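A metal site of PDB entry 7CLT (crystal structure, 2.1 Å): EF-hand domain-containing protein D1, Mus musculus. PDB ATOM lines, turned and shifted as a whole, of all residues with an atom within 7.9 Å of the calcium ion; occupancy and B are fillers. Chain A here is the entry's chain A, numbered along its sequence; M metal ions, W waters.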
ATOM      1  N   PHE A  37     -22.896 -24.620 -25.327  1.00  0.00           N
ATOM      2  CA  PHE A  37     -21.528 -24.332 -24.923  1.00  0.00           C
ATOM      3  C   PHE A  37     -20.974 -25.413 -24.004  1.00  0.00           C
ATOM      4  O   PHE A  37     -19.854 -25.921 -24.219  1.00  0.00           O
ATOM      5  CB  PHE A  37     -21.437 -22.977 -24.245  1.00  0.00           C
ATOM      6  CG  PHE A  37     -20.022 -22.550 -23.958  1.00  0.00           C
ATOM      7  CD1 PHE A  37     -19.271 -21.892 -24.932  1.00  0.00           C
ATOM      8  CD2 PHE A  37     -19.438 -22.821 -22.743  1.00  0.00           C
ATOM      9  CE1 PHE A  37     -17.971 -21.520 -24.679  1.00  0.00           C
ATOM     10  CE2 PHE A  37     -18.137 -22.440 -22.479  1.00  0.00           C
ATOM     11  CZ  PHE A  37     -17.399 -21.777 -23.448  1.00  0.00           C
ATOM     12  N   TYR A  40     -20.109 -28.899 -25.804  1.00  0.00           N
ATOM     13  CA  TYR A  40     -18.945 -29.054 -26.647  1.00  0.00           C
ATOM     14  C   TYR A  40     -17.638 -28.628 -25.971  1.00  0.00           C
ATOM     15  O   TYR A  40     -16.561 -28.849 -26.536  1.00  0.00           O
ATOM     16  CB  TYR A  40     -19.164 -28.275 -27.937  1.00  0.00           C
ATOM     17  CG  TYR A  40     -20.268 -28.896 -28.784  1.00  0.00           C
ATOM     18  CD1 TYR A  40     -21.512 -28.284 -28.911  1.00  0.00           C
ATOM     19  CD2 TYR A  40     -20.054 -30.095 -29.453  1.00  0.00           C
ATOM     20  CE1 TYR A  40     -22.505 -28.848 -29.700  1.00  0.00           C
ATOM     21  CE2 TYR A  40     -21.037 -30.669 -30.226  1.00  0.00           C
ATOM     22  CZ  TYR A  40     -22.260 -30.050 -30.350  1.00  0.00           C
ATOM     23  OH  TYR A  40     -23.212 -30.654 -31.137  1.00  0.00           O
ATOM     24  N   ASP A  41     -17.708 -28.056 -24.758  1.00  0.00           N
ATOM     25  CA  ASP A  41     -16.513 -27.861 -23.936  1.00  0.00           C
ATOM     26  C   ASP A  41     -16.211 -29.171 -23.214  1.00  0.00           C
ATOM     27  O   ASP A  41     -16.478 -29.342 -22.019  1.00  0.00           O
ATOM     28  CB  ASP A  41     -16.716 -26.719 -22.929  1.00  0.00           C
ATOM     29  CG  ASP A  41     -15.472 -26.473 -22.069  1.00  0.00           C
ATOM     30  OD1 ASP A  41     -15.559 -25.721 -21.072  1.00  0.00           O
ATOM     31  OD2 ASP A  41     -14.406 -27.029 -22.395  1.00  0.00           O
ATOM     32  N   ALA A  42     -15.610 -30.110 -23.965  1.00  0.00           N
ATOM     33  CA  ALA A  42     -15.377 -31.447 -23.433  1.00  0.00           C
ATOM     34  C   ALA A  42     -14.568 -31.398 -22.144  1.00  0.00           C
ATOM     35  O   ALA A  42     -14.986 -31.921 -21.110  1.00  0.00           O
ATOM     36  CB  ALA A  42     -14.684 -32.315 -24.475  1.00  0.00           C
ATOM     37  N   GLY A  43     -13.408 -30.740 -22.192  1.00  0.00           N
ATOM     38  CA  GLY A  43     -12.530 -30.671 -21.037  1.00  0.00           C
ATOM     39  C   GLY A  43     -13.073 -29.886 -19.867  1.00  0.00           C
ATOM     40  O   GLY A  43     -12.479 -29.919 -18.790  1.00  0.00           O
ATOM     41  N   ARG A  44     -14.175 -29.156 -20.064  1.00  0.00           N
ATOM     42  CA  ARG A  44     -14.800 -28.377 -19.002  1.00  0.00           C
ATOM     43  C   ARG A  44     -13.827 -27.360 -18.399  1.00  0.00           C
ATOM     44  O   ARG A  44     -13.835 -27.100 -17.189  1.00  0.00           O
ATOM     45  CB  ARG A  44     -15.400 -29.283 -17.934  1.00  0.00           C
ATOM     46  CG  ARG A  44     -16.278 -30.400 -18.518  1.00  0.00           C
ATOM     47  CD  ARG A  44     -17.645 -30.402 -17.875  1.00  0.00           C
ATOM     48  NE  ARG A  44     -17.549 -30.620 -16.430  1.00  0.00           N
ATOM     49  CZ  ARG A  44     -18.242 -31.540 -15.756  1.00  0.00           C
ATOM     50  NH1 ARG A  44     -19.096 -32.334 -16.402  1.00  0.00           N
ATOM     51  NH2 ARG A  44     -18.086 -31.665 -14.447  1.00  0.00           N
ATOM     52  N   ASP A  45     -12.977 -26.770 -19.245  1.00  0.00           N
ATOM     53  CA  ASP A  45     -12.132 -25.668 -18.800  1.00  0.00           C
ATOM     54  C   ASP A  45     -12.804 -24.314 -18.950  1.00  0.00           C
ATOM     55  O   ASP A  45     -12.199 -23.296 -18.598  1.00  0.00           O
ATOM     56  CB  ASP A  45     -10.814 -25.665 -19.574  1.00  0.00           C
ATOM     57  CG  ASP A  45     -10.995 -25.487 -21.075  1.00  0.00           C
ATOM     58  OD1 ASP A  45      -9.989 -25.225 -21.748  1.00  0.00           O
ATOM     59  OD2 ASP A  45     -12.143 -25.601 -21.586  1.00  0.00           O
ATOM     60  N   GLY A  46     -14.035 -24.277 -19.449  1.00  0.00           N
ATOM     61  CA  GLY A  46     -14.731 -23.022 -19.683  1.00  0.00           C
ATOM     62  C   GLY A  46     -14.487 -22.393 -21.040  1.00  0.00           C
ATOM     63  O   GLY A  46     -14.928 -21.246 -21.265  1.00  0.00           O
ATOM     64  N   PHE A  47     -13.797 -23.085 -21.949  1.00  0.00           N
ATOM     65  CA  PHE A  47     -13.483 -22.600 -23.280  1.00  0.00           C
ATOM     66  C   PHE A  47     -13.846 -23.663 -24.303  1.00  0.00           C
ATOM     67  O   PHE A  47     -13.849 -24.860 -24.001  1.00  0.00           O
ATOM     68  CB  PHE A  47     -11.994 -22.244 -23.405  1.00  0.00           C
ATOM     69  CG  PHE A  47     -11.514 -21.275 -22.360  1.00  0.00           C
ATOM     70  CD1 PHE A  47     -10.738 -21.719 -21.289  1.00  0.00           C
ATOM     71  CD2 PHE A  47     -11.874 -19.930 -22.420  1.00  0.00           C
ATOM     72  CE1 PHE A  47     -10.312 -20.827 -20.325  1.00  0.00           C
ATOM     73  CE2 PHE A  47     -11.439 -19.026 -21.448  1.00  0.00           C
ATOM     74  CZ  PHE A  47     -10.660 -19.488 -20.390  1.00  0.00           C
ATOM     75  N   ILE A  48     -14.175 -23.230 -25.511  1.00  0.00           N
ATOM     76  CA  ILE A  48     -14.228 -24.124 -26.678  1.00  0.00           C
ATOM     77  C   ILE A  48     -12.984 -23.801 -27.506  1.00  0.00           C
ATOM     78  O   ILE A  48     -12.834 -22.681 -28.024  1.00  0.00           O
ATOM     79  CB  ILE A  48     -15.531 -23.975 -27.463  1.00  0.00           C
ATOM     80  CG1 ILE A  48     -16.691 -24.550 -26.632  1.00  0.00           C
ATOM     81  CG2 ILE A  48     -15.428 -24.708 -28.832  1.00  0.00           C
ATOM     82  CD1 ILE A  48     -18.054 -24.405 -27.243  1.00  0.00           C
ATOM     83  N   ASP A  49     -12.056 -24.743 -27.558  1.00  0.00           N
ATOM     84  CA  ASP A  49     -10.805 -24.534 -28.247  1.00  0.00           C
ATOM     85  C   ASP A  49     -10.927 -25.052 -29.671  1.00  0.00           C
ATOM     86  O   ASP A  49     -11.995 -25.502 -30.098  1.00  0.00           O
ATOM     87  CB  ASP A  49      -9.637 -25.190 -27.477  1.00  0.00           C
ATOM     88  CG  ASP A  49      -9.824 -26.728 -27.288  1.00  0.00           C
ATOM     89  OD1 ASP A  49     -10.325 -27.421 -28.197  1.00  0.00           O
ATOM     90  OD2 ASP A  49      -9.414 -27.255 -26.217  1.00  0.00           O
ATOM     91  N   LEU A  50      -9.833 -24.991 -30.427  1.00  0.00           N
ATOM     92  CA  LEU A  50      -9.915 -25.280 -31.851  1.00  0.00           C
ATOM     93  C   LEU A  50     -10.387 -26.716 -32.103  1.00  0.00           C
ATOM     94  O   LEU A  50     -11.232 -26.955 -32.959  1.00  0.00           O
ATOM     95  CB  LEU A  50      -8.563 -25.001 -32.500  1.00  0.00           C
ATOM     96  CG  LEU A  50      -8.447 -25.159 -34.015  1.00  0.00           C
ATOM     97  CD1 LEU A  50      -9.312 -24.174 -34.676  1.00  0.00           C
ATOM     98  CD2 LEU A  50      -7.014 -24.884 -34.415  1.00  0.00           C
ATOM     99  N   GLU A  52     -12.161 -28.687 -29.996  1.00  0.00           N
ATOM    100  CA  GLU A  52     -13.567 -28.838 -29.630  1.00  0.00           C
ATOM    101  C   GLU A  52     -14.487 -28.182 -30.661  1.00  0.00           C
ATOM    102  O   GLU A  52     -15.564 -28.716 -30.961  1.00  0.00           O
ATOM    103  CB  GLU A  52     -13.792 -28.274 -28.225  1.00  0.00           C
ATOM    104  CG  GLU A  52     -12.961 -29.011 -27.154  1.00  0.00           C
ATOM    105  CD  GLU A  52     -12.910 -28.280 -25.836  1.00  0.00           C
ATOM    106  OE1 GLU A  52     -12.636 -27.062 -25.845  1.00  0.00           O
ATOM    107  OE2 GLU A  52     -13.142 -28.896 -24.775  1.00  0.00           O
ATOM    108  N   LEU A  53     -14.078 -27.055 -31.248  1.00  0.00           N
ATOM    109  CA  LEU A  53     -14.863 -26.462 -32.327  1.00  0.00           C
ATOM    110  C   LEU A  53     -14.923 -27.403 -33.537  1.00  0.00           C
ATOM    111  O   LEU A  53     -15.979 -27.546 -34.173  1.00  0.00           O
ATOM    112  CB  LEU A  53     -14.256 -25.118 -32.750  1.00  0.00           C
ATOM    113  CG  LEU A  53     -15.092 -24.376 -33.798  1.00  0.00           C
ATOM    114  CD1 LEU A  53     -16.506 -24.113 -33.257  1.00  0.00           C
ATOM    115  CD2 LEU A  53     -14.406 -23.077 -34.181  1.00  0.00           C
ATOM    116  N   LYS A  83      -9.092 -19.303 -28.373  1.00  0.00           N
ATOM    117  CA  LYS A  83     -10.163 -20.164 -27.879  1.00  0.00           C
ATOM    118  C   LYS A  83     -11.356 -19.289 -27.533  1.00  0.00           C
ATOM    119  O   LYS A  83     -11.233 -18.074 -27.363  1.00  0.00           O
ATOM    120  CB  LYS A  83      -9.724 -20.973 -26.647  1.00  0.00           C
ATOM    121  CG  LYS A  83      -9.459 -20.117 -25.416  1.00  0.00           C
ATOM    122  CD  LYS A  83      -8.519 -20.876 -24.476  1.00  0.00           C
ATOM    123  CE  LYS A  83      -8.176 -20.055 -23.258  1.00  0.00           C
ATOM    124  NZ  LYS A  83      -7.453 -20.869 -22.257  1.00  0.00           N
ATOM    125  N   LEU A  84     -12.520 -19.916 -27.428  1.00  0.00           N
ATOM    126  CA  LEU A  84     -13.768 -19.188 -27.243  1.00  0.00           C
ATOM    127  C   LEU A  84     -14.234 -19.328 -25.805  1.00  0.00           C
ATOM    128  O   LEU A  84     -14.550 -20.447 -25.361  1.00  0.00           O
ATOM    129  CB  LEU A  84     -14.848 -19.697 -28.177  1.00  0.00           C
ATOM    130  CG  LEU A  84     -14.600 -19.585 -29.681  1.00  0.00           C
ATOM    131  CD1 LEU A  84     -15.679 -20.362 -30.419  1.00  0.00           C
ATOM    132  CD2 LEU A  84     -14.554 -18.133 -30.100  1.00  0.00           C
HETATM  133 CA    CA M   1     -12.605 -26.647 -23.572  1.00  0.00          CA
HETATM  134  O   HOH W   1     -11.015 -28.252 -22.619  1.00  0.00           O
HETATM  135  O   HOH W   2     -10.634 -25.848 -24.245  1.00  0.00           O
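The calcium ion is bound by OD2 of Asp 41 (2.2 Å), O of Phe 47 (2.2 Å), water W2 (2.2 Å), OD2 of Asp 45 (2.3 Å), OE1 of Glu 52 (2.3 Å), water W1 (2.5 Å) and OE2 of Glu 52 (2.6 Å). The calcium ion has seven donor atoms within binding distance.
Within 4 Å of the calcium ion: Asp 41, Asp 45, Phe 47 and Glu 52. The nearest printed residue that does not touch the calcium ion is Asp 49 (4.2 Å).
Water W2 lies within hydrogen-bond range of the side-chain carboxylate of Asp 45 and the side-chain carboxylate of Asp 49. Water W1 bridges OD1 of Asp 45 and N of Gly 43.
The backbone NH (N) of Gly 46 lies within hydrogen-bond range of the side-chain carboxylate (OD1) of Asp 41, 2.7 Å away. The backbone NH (N) of Arg 44 sits close to the side-chain carboxylate (OD2) of Asp 41 (3.2 Å). OD1 of Asp 49 sits at hydrogen-bond distance from N of Glu 52. OE2 of Glu 52 sits close to N of Gly 43 (3.2 Å). The backbone NH of Ala 42 lies close to the side-chain carboxylate of Glu 52 (2.9 Å).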
